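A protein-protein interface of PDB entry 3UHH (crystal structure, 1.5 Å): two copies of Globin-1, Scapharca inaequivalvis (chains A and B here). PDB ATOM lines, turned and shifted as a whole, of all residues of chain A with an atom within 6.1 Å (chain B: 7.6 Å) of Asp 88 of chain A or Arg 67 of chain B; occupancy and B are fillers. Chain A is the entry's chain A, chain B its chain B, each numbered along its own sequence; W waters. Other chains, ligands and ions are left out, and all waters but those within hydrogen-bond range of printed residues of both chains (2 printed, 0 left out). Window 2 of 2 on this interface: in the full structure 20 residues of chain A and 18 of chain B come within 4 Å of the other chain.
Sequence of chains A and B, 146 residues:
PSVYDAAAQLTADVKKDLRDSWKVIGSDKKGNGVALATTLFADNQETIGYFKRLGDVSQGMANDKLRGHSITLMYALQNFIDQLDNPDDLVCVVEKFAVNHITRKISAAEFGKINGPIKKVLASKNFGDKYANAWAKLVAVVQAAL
The backbone carbonyl oxygen (O) of Met 61 of chain B sits at hydrogen-bond distance from the guanidinium group (NH1) of Arg 67 of chain B (2.9 Å).
The backbone carbonyl oxygen (O) of Gly 68 of chain B is in hydrogen-bond range of the side-chain hydroxyl (OG1) of Thr 72 of chain B.
The side-chain amide oxygen (OD1) of Asn 86 of chain A is in hydrogen-bond range of the backbone NH (N) of Asp 88 of chain A (3.0 Å).
O of Asp 89 of chain A is in hydrogen-bond range of SG of Cys 92 of chain A (3.4 Å).
The side-chain amide oxygen (OD1) of Asn 86 of chain A sits at hydrogen-bond distance from the backbone NH (N) of Asp 89 of chain A (3.2 Å).
OD1 of Asp 89 of chain A lies within salt-bridge range of NE of Arg 67 of chain B.
The side-chain carboxylate (OD2) of Asp 89 of chain A is in salt-bridge range of the side-chain amino group (NZ) of Lys 30 of chain B.
The side-chain sulfur (SG) of Cys 92 of chain A lies within hydrogen-bond range of the backbone NH (N) of Gly 68 of chain B, at 3.5 Å.
The backbone carbonyl oxygen (O) of Asp 88 of chain A lies within hydrogen-bond range of the guanidinium group (NH2) of Arg 67 of chain B (3.3 Å).
Water W2 lies within hydrogen-bond range of OD1 of Asp 89 of chain A (2.7 Å) and NZ of Lys 30 of chain B (3.5 Å).
Water W1 bridges O of Asp 88 of chain A and NH2 of Arg 67 of chain B.
Among the printed residues, merely in contact across the chains: Cys 92 of chain A with Asp 64 of chain B, Cys 92 of chain A with Arg 67 of chain B and Val 93 of chain A with Ile 71 of chain B.
Hydrophobic or aromatic side chains of chain A that line the printed part of chain B: Val 93.
Hydrophobic or aromatic side chains of chain B that line the printed part of chain A: Ile 71.
Among the printed residues, 7 pairs touch across the chains.
Among the printed residues, Asp or Glu carboxylates within 4 Å of a Lys or Arg side-chain nitrogen of the other chain: Asp 89 of chain A with Lys 30 of chain B (2.7 Å) and Asp 89 of chain A with Arg 67 of chain B (2.9 Å).
Asn 86 of chain A touches none of the printed residues of chain B.
Asp 88 of chain A touches just one residue of chain B: Arg 67.
Of the printed residues of chain B, Asp 89 of chain A touches Lys 30 (2.7 Å) and Arg 67 (2.9 Å).
Of the printed residues of chain A, Lys 30 of chain B touches Asp 89 (2.7 Å).
Ala 62 of chain B touches none of the printed residues of chain A.
Arg 67 of chain B touches three residues of chain A.
The nearest printed residue of chain B that does not touch Asp 88 of chain A is Asp 64 of chain B (6.1 Å).
The nearest printed residue of chain A that does not touch Arg 67 of chain B is Val 93 of chain A (5.3 Å).
The nearest printed residue of chain A that does not touch Ile 71 of chain B is Cys 92 of chain A (4.5 Å).
No position is printed for both chains.
Of the 7 pairs that touch across the chains among the printed residues, none has its exchanged pair printed and touching as well.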
ATOM      1  N   TYR A   4       7.944  22.107  37.721  1.00  0.00           N
ATOM      2  CA  TYR A   4       8.497  23.189  36.919  1.00  0.00           C
ATOM      3  C   TYR A   4       9.197  24.221  37.795  1.00  0.00           C
ATOM      4  O   TYR A   4      10.246  24.747  37.426  1.00  0.00           O
ATOM      5  CB  TYR A   4       7.388  23.840  36.090  1.00  0.00           C
ATOM      6  CG  TYR A   4       6.822  22.894  35.059  1.00  0.00           C
ATOM      7  CD1 TYR A   4       7.527  22.604  33.892  1.00  0.00           C
ATOM      8  CD2 TYR A   4       5.617  22.227  35.284  1.00  0.00           C
ATOM      9  CE1 TYR A   4       7.052  21.673  32.975  1.00  0.00           C
ATOM     10  CE2 TYR A   4       5.134  21.291  34.376  1.00  0.00           C
ATOM     11  CZ  TYR A   4       5.858  21.018  33.225  1.00  0.00           C
ATOM     12  OH  TYR A   4       5.393  20.083  32.332  1.00  0.00           O
ATOM     13  N   ASN A  86      18.026  21.676  28.860  1.00  0.00           N
ATOM     14  CA  ASN A  86      16.639  21.921  28.477  1.00  0.00           C
ATOM     15  C   ASN A  86      15.639  21.504  29.558  1.00  0.00           C
ATOM     16  O   ASN A  86      15.366  20.319  29.741  1.00  0.00           O
ATOM     17  CB  ASN A  86      16.336  21.169  27.180  1.00  0.00           C
ATOM     18  CG  ASN A  86      15.026  21.590  26.553  1.00  0.00           C
ATOM     19  OD1 ASN A  86      13.991  21.632  27.215  1.00  0.00           O
ATOM     20  ND2 ASN A  86      15.064  21.898  25.260  1.00  0.00           N
ATOM     21  N   PRO A  87      15.067  22.482  30.276  1.00  0.00           N
ATOM     22  CA  PRO A  87      14.093  22.234  31.345  1.00  0.00           C
ATOM     23  C   PRO A  87      12.906  21.355  30.946  1.00  0.00           C
ATOM     24  O   PRO A  87      12.486  20.483  31.709  1.00  0.00           O
ATOM     25  CB  PRO A  87      13.658  23.642  31.741  1.00  0.00           C
ATOM     26  CG  PRO A  87      14.902  24.439  31.517  1.00  0.00           C
ATOM     27  CD  PRO A  87      15.370  23.921  30.176  1.00  0.00           C
ATOM     28  N   ASP A  88      12.363  21.585  29.756  1.00  0.00           N
ATOM     29  CA  ASP A  88      11.223  20.808  29.288  1.00  0.00           C
ATOM     30  C   ASP A  88      11.564  19.335  29.112  1.00  0.00           C
ATOM     31  O   ASP A  88      10.718  18.470  29.333  1.00  0.00           O
ATOM     32  CB  ASP A  88      10.693  21.372  27.968  1.00  0.00           C
ATOM     33  CG  ASP A  88      10.157  22.780  28.112  1.00  0.00           C
ATOM     34  OD1 ASP A  88       9.261  22.992  28.956  1.00  0.00           O
ATOM     35  OD2 ASP A  88      10.629  23.676  27.381  1.00  0.00           O
ATOM     36  N   ASP A  89      12.795  19.045  28.707  1.00  0.00           N
ATOM     37  CA  ASP A  89      13.191  17.655  28.530  1.00  0.00           C
ATOM     38  C   ASP A  89      13.527  17.024  29.872  1.00  0.00           C
ATOM     39  O   ASP A  89      13.299  15.836  30.074  1.00  0.00           O
ATOM     40  CB  ASP A  89      14.380  17.540  27.577  1.00  0.00           C
ATOM     41  CG  ASP A  89      14.014  17.899  26.150  1.00  0.00           C
ATOM     42  OD1 ASP A  89      12.827  17.749  25.791  1.00  0.00           O
ATOM     43  OD2 ASP A  89      14.908  18.318  25.390  1.00  0.00           O
ATOM     44  N   LEU A  90      14.066  17.814  30.793  1.00  0.00           N
ATOM     45  CA  LEU A  90      14.385  17.283  32.110  1.00  0.00           C
ATOM     46  C   LEU A  90      13.079  16.884  32.789  1.00  0.00           C
ATOM     47  O   LEU A  90      12.967  15.808  33.381  1.00  0.00           O
ATOM     48  CB  LEU A  90      15.101  18.338  32.959  1.00  0.00           C
ATOM     49  CG  LEU A  90      15.372  17.949  34.414  1.00  0.00           C
ATOM     50  CD1 LEU A  90      16.319  16.760  34.469  1.00  0.00           C
ATOM     51  CD2 LEU A  90      15.970  19.136  35.154  1.00  0.00           C
ATOM     52  N   VAL A  91      12.084  17.756  32.693  1.00  0.00           N
ATOM     53  CA  VAL A  91      10.799  17.480  33.316  1.00  0.00           C
ATOM     54  C   VAL A  91      10.137  16.208  32.789  1.00  0.00           C
ATOM     55  O   VAL A  91       9.624  15.413  33.571  1.00  0.00           O
ATOM     56  CB  VAL A  91       9.819  18.662  33.139  1.00  0.00           C
ATOM     57  CG1 VAL A  91       8.421  18.258  33.598  1.00  0.00           C
ATOM     58  CG2 VAL A  91      10.298  19.853  33.956  1.00  0.00           C
ATOM     59  N   CYS A  92      10.159  15.994  31.475  1.00  0.00           N
ATOM     60  CA  CYS A  92       9.505  14.803  30.947  1.00  0.00           C
ATOM     61  C   CYS A  92      10.189  13.487  31.324  1.00  0.00           C
ATOM     62  O   CYS A  92       9.520  12.469  31.474  1.00  0.00           O
ATOM     63  CB  CYS A  92       9.293  14.908  29.423  1.00  0.00           C
ATOM     64  SG  CYS A  92      10.688  14.570  28.349  1.00  0.00           S
ATOM     65  N   VAL A  93      11.512  13.498  31.478  1.00  0.00           N
ATOM     66  CA  VAL A  93      12.211  12.275  31.859  1.00  0.00           C
ATOM     67  C   VAL A  93      12.038  12.042  33.358  1.00  0.00           C
ATOM     68  O   VAL A  93      11.959  10.901  33.810  1.00  0.00           O
ATOM     69  CB  VAL A  93      13.720  12.328  31.518  1.00  0.00           C
ATOM     70  CG1 VAL A  93      13.912  12.310  30.008  1.00  0.00           C
ATOM     71  CG2 VAL A  93      14.355  13.563  32.123  1.00  0.00           C
ATOM     72  N   LYS B  29      19.884  11.523  21.259  1.00  0.00           N
ATOM     73  CA  LYS B  29      18.934  10.608  21.869  1.00  0.00           C
ATOM     74  C   LYS B  29      17.479  11.032  21.744  1.00  0.00           C
ATOM     75  O   LYS B  29      16.610  10.194  21.522  1.00  0.00           O
ATOM     76  CB  LYS B  29      19.314  10.375  23.332  1.00  0.00           C
ATOM     77  CG  LYS B  29      20.658   9.669  23.473  1.00  0.00           C
ATOM     78  CD  LYS B  29      20.985   9.348  24.919  1.00  0.00           C
ATOM     79  CE  LYS B  29      22.177   8.408  25.027  1.00  0.00           C
ATOM     80  NZ  LYS B  29      23.421   8.983  24.450  1.00  0.00           N
ATOM     81  N   LYS B  30      17.204  12.325  21.872  1.00  0.00           N
ATOM     82  CA  LYS B  30      15.829  12.798  21.751  1.00  0.00           C
ATOM     83  C   LYS B  30      15.312  12.621  20.324  1.00  0.00           C
ATOM     84  O   LYS B  30      14.260  12.017  20.102  1.00  0.00           O
ATOM     85  CB  LYS B  30      15.724  14.272  22.159  1.00  0.00           C
ATOM     86  CG  LYS B  30      14.336  14.859  21.941  1.00  0.00           C
ATOM     87  CD  LYS B  30      14.157  16.213  22.623  1.00  0.00           C
ATOM     88  CE  LYS B  30      15.086  17.276  22.068  1.00  0.00           C
ATOM     89  NZ  LYS B  30      14.805  18.604  22.685  1.00  0.00           N
ATOM     90  N   GLY B  31      16.065  13.143  19.360  1.00  0.00           N
ATOM     91  CA  GLY B  31      15.665  13.049  17.968  1.00  0.00           C
ATOM     92  C   GLY B  31      15.564  11.636  17.425  1.00  0.00           C
ATOM     93  O   GLY B  31      14.553  11.268  16.824  1.00  0.00           O
ATOM     94  N   GLY B  33      15.562   8.842  19.244  1.00  0.00           N
ATOM     95  CA  GLY B  33      14.729   8.008  20.090  1.00  0.00           C
ATOM     96  C   GLY B  33      13.279   8.121  19.655  1.00  0.00           C
ATOM     97  O   GLY B  33      12.573   7.120  19.539  1.00  0.00           O
ATOM     98  N   VAL B  34      12.831   9.348  19.407  1.00  0.00           N
ATOM     99  CA  VAL B  34      11.460   9.573  18.972  1.00  0.00           C
ATOM    100  C   VAL B  34      11.257   9.028  17.556  1.00  0.00           C
ATOM    101  O   VAL B  34      10.175   8.547  17.225  1.00  0.00           O
ATOM    102  CB  VAL B  34      11.100  11.077  19.010  1.00  0.00           C
ATOM    103  CG1 VAL B  34       9.716  11.302  18.408  1.00  0.00           C
ATOM    104  CG2 VAL B  34      11.129  11.574  20.450  1.00  0.00           C
ATOM    105  N   LEU B  54       1.181   6.322  27.270  1.00  0.00           N
ATOM    106  CA  LEU B  54       1.790   7.481  26.630  1.00  0.00           C
ATOM    107  C   LEU B  54       0.803   8.442  25.969  1.00  0.00           C
ATOM    108  O   LEU B  54       1.201   9.503  25.490  1.00  0.00           O
ATOM    109  CB  LEU B  54       2.816   7.020  25.591  1.00  0.00           C
ATOM    110  CG  LEU B  54       3.905   6.054  26.067  1.00  0.00           C
ATOM    111  CD1 LEU B  54       4.850   5.749  24.907  1.00  0.00           C
ATOM    112  CD2 LEU B  54       4.672   6.656  27.231  1.00  0.00           C
ATOM    113  N   GLY B  60       3.797  12.725  18.368  1.00  0.00           N
ATOM    114  CA  GLY B  60       5.243  12.747  18.243  1.00  0.00           C
ATOM    115  C   GLY B  60       6.002  13.506  19.318  1.00  0.00           C
ATOM    116  O   GLY B  60       5.748  13.348  20.511  1.00  0.00           O
ATOM    117  N   MET B  61       6.941  14.332  18.873  1.00  0.00           N
ATOM    118  CA  MET B  61       7.792  15.128  19.752  1.00  0.00           C
ATOM    119  C   MET B  61       7.017  15.998  20.740  1.00  0.00           C
ATOM    120  O   MET B  61       7.486  16.248  21.853  1.00  0.00           O
ATOM    121  CB  MET B  61       8.705  16.012  18.897  1.00  0.00           C
ATOM    122  CG  MET B  61       9.870  16.628  19.644  1.00  0.00           C
ATOM    123  SD  MET B  61      11.014  15.386  20.271  1.00  0.00           S
ATOM    124  CE  MET B  61      11.884  14.929  18.774  1.00  0.00           C
ATOM    125  N   ALA B  62       5.836  16.454  20.332  1.00  0.00           N
ATOM    126  CA  ALA B  62       5.002  17.306  21.174  1.00  0.00           C
ATOM    127  C   ALA B  62       4.449  16.575  22.392  1.00  0.00           C
ATOM    128  O   ALA B  62       4.126  17.200  23.400  1.00  0.00           O
ATOM    129  CB  ALA B  62       3.856  17.889  20.354  1.00  0.00           C
ATOM    130  N   ASN B  63       4.334  15.254  22.292  1.00  0.00           N
ATOM    131  CA  ASN B  63       3.826  14.431  23.387  1.00  0.00           C
ATOM    132  C   ASN B  63       4.957  14.265  24.403  1.00  0.00           C
ATOM    133  O   ASN B  63       5.927  13.552  24.147  1.00  0.00           O
ATOM    134  CB  ASN B  63       3.405  13.063  22.844  1.00  0.00           C
ATOM    135  CG  ASN B  63       2.773  12.185  23.898  1.00  0.00           C
ATOM    136  OD1 ASN B  63       3.186  12.194  25.056  1.00  0.00           O
ATOM    137  ND2 ASN B  63       1.776  11.403  23.500  1.00  0.00           N
ATOM    138  N   ASP B  64       4.824  14.920  25.554  1.00  0.00           N
ATOM    139  CA  ASP B  64       5.847  14.858  26.592  1.00  0.00           C
ATOM    140  C   ASP B  64       6.087  13.454  27.145  1.00  0.00           C
ATOM    141  O   ASP B  64       7.219  13.098  27.468  1.00  0.00           O
ATOM    142  CB  ASP B  64       5.491  15.817  27.733  1.00  0.00           C
ATOM    143  CG  ASP B  64       4.146  15.512  28.356  1.00  0.00           C
ATOM    144  OD1 ASP B  64       3.145  15.428  27.613  1.00  0.00           O
ATOM    145  OD2 ASP B  64       4.087  15.363  29.593  1.00  0.00           O
ATOM    146  N   LYS B  65       5.028  12.659  27.253  1.00  0.00           N
ATOM    147  CA  LYS B  65       5.165  11.301  27.765  1.00  0.00           C
ATOM    148  C   LYS B  65       5.931  10.434  26.772  1.00  0.00           C
ATOM    149  O   LYS B  65       6.751   9.604  27.165  1.00  0.00           O
ATOM    150  CB  LYS B  65       3.794  10.684  28.060  1.00  0.00           C
ATOM    151  CG  LYS B  65       3.162  11.203  29.340  1.00  0.00           C
ATOM    152  CD  LYS B  65       1.852  10.498  29.642  1.00  0.00           C
ATOM    153  CE  LYS B  65       1.279  10.968  30.966  1.00  0.00           C
ATOM    154  NZ  LYS B  65       1.084  12.442  30.975  1.00  0.00           N
ATOM    155  N   LEU B  66       5.665  10.635  25.484  1.00  0.00           N
ATOM    156  CA  LEU B  66       6.350   9.874  24.448  1.00  0.00           C
ATOM    157  C   LEU B  66       7.812  10.296  24.390  1.00  0.00           C
ATOM    158  O   LEU B  66       8.705   9.468  24.216  1.00  0.00           O
ATOM    159  CB  LEU B  66       5.689  10.117  23.087  1.00  0.00           C
ATOM    160  CG  LEU B  66       6.365   9.497  21.860  1.00  0.00           C
ATOM    161  CD1 LEU B  66       6.469   7.986  22.019  1.00  0.00           C
ATOM    162  CD2 LEU B  66       5.563   9.845  20.618  1.00  0.00           C
ATOM    163  N   ARG B  67       8.053  11.594  24.543  1.00  0.00           N
ATOM    164  CA  ARG B  67       9.414  12.108  24.505  1.00  0.00           C
ATOM    165  C   ARG B  67      10.221  11.556  25.679  1.00  0.00           C
ATOM    166  O   ARG B  67      11.359  11.129  25.505  1.00  0.00           O
ATOM    167  CB  ARG B  67       9.403  13.641  24.539  1.00  0.00           C
ATOM    168  CG  ARG B  67      10.698  14.267  24.047  1.00  0.00           C
ATOM    169  CD  ARG B  67      10.574  15.773  23.814  1.00  0.00           C
ATOM    170  NE  ARG B  67      10.341  16.521  25.048  1.00  0.00           N
ATOM    171  CZ  ARG B  67       9.171  17.041  25.403  1.00  0.00           C
ATOM    172  NH1 ARG B  67       8.111  16.904  24.615  1.00  0.00           N
ATOM    173  NH2 ARG B  67       9.057  17.702  26.548  1.00  0.00           N
ATOM    174  N   GLY B  68       9.626  11.556  26.868  1.00  0.00           N
ATOM    175  CA  GLY B  68      10.322  11.040  28.036  1.00  0.00           C
ATOM    176  C   GLY B  68      10.633   9.565  27.876  1.00  0.00           C
ATOM    177  O   GLY B  68      11.709   9.098  28.245  1.00  0.00           O
ATOM    178  N   HIS B  69       9.677   8.828  27.325  1.00  0.00           N
ATOM    179  CA  HIS B  69       9.842   7.398  27.096  1.00  0.00           C
ATOM    180  C   HIS B  69      10.954   7.128  26.082  1.00  0.00           C
ATOM    181  O   HIS B  69      11.813   6.276  26.300  1.00  0.00           O
ATOM    182  CB  HIS B  69       8.534   6.801  26.567  1.00  0.00           C
ATOM    183  CG  HIS B  69       8.680   5.415  26.021  1.00  0.00           C
ATOM    184  ND1 HIS B  69       8.726   4.316  26.844  1.00  0.00           N
ATOM    185  CD2 HIS B  69       8.818   5.015  24.731  1.00  0.00           C
ATOM    186  CE1 HIS B  69       8.892   3.278  26.047  1.00  0.00           C
ATOM    187  NE2 HIS B  69       8.955   3.651  24.756  1.00  0.00           N
ATOM    188  N   SER B  70      10.923   7.862  24.976  1.00  0.00           N
ATOM    189  CA  SER B  70      11.896   7.697  23.904  1.00  0.00           C
ATOM    190  C   SER B  70      13.324   8.029  24.309  1.00  0.00           C
ATOM    191  O   SER B  70      14.262   7.338  23.915  1.00  0.00           O
ATOM    192  CB  SER B  70      11.490   8.548  22.702  1.00  0.00           C
ATOM    193  OG  SER B  70      10.201   8.172  22.246  1.00  0.00           O
ATOM    194  N   ILE B  71      13.499   9.099  25.075  1.00  0.00           N
ATOM    195  CA  ILE B  71      14.836   9.461  25.524  1.00  0.00           C
ATOM    196  C   ILE B  71      15.359   8.353  26.438  1.00  0.00           C
ATOM    197  O   ILE B  71      16.502   7.917  26.313  1.00  0.00           O
ATOM    198  CB  ILE B  71      14.828  10.799  26.296  1.00  0.00           C
ATOM    199  CG1 ILE B  71      14.530  11.951  25.331  1.00  0.00           C
ATOM    200  CG2 ILE B  71      16.172  11.015  26.995  1.00  0.00           C
ATOM    201  CD1 ILE B  71      14.294  13.276  26.027  1.00  0.00           C
ATOM    202  N   THR B  72      14.508   7.890  27.350  1.00  0.00           N
ATOM    203  CA  THR B  72      14.893   6.841  28.285  1.00  0.00           C
ATOM    204  C   THR B  72      15.223   5.530  27.565  1.00  0.00           C
ATOM    205  O   THR B  72      16.129   4.799  27.971  1.00  0.00           O
ATOM    206  CB  THR B  72      13.781   6.626  29.331  1.00  0.00           C
ATOM    207  OG1 THR B  72      13.545   7.863  30.016  1.00  0.00           O
ATOM    208  CG2 THR B  72      14.190   5.571  30.347  1.00  0.00           C
ATOM    209  N   LEU B  73      14.502   5.238  26.487  1.00  0.00           N
ATOM    210  CA  LEU B  73      14.768   4.022  25.732  1.00  0.00           C
ATOM    211  C   LEU B  73      16.203   4.057  25.198  1.00  0.00           C
ATOM    212  O   LEU B  73      16.903   3.041  25.193  1.00  0.00           O
ATOM    213  CB  LEU B  73      13.767   3.891  24.574  1.00  0.00           C
ATOM    214  CG  LEU B  73      13.914   2.696  23.623  1.00  0.00           C
ATOM    215  CD1 LEU B  73      12.566   2.376  22.995  1.00  0.00           C
ATOM    216  CD2 LEU B  73      14.953   3.002  22.554  1.00  0.00           C
HETATM  217  O   HOH W   1       8.031  18.568  29.026  1.00  0.00           O
HETATM  218  O   HOH W   2      11.790  19.607  24.137  1.00  0.00           O
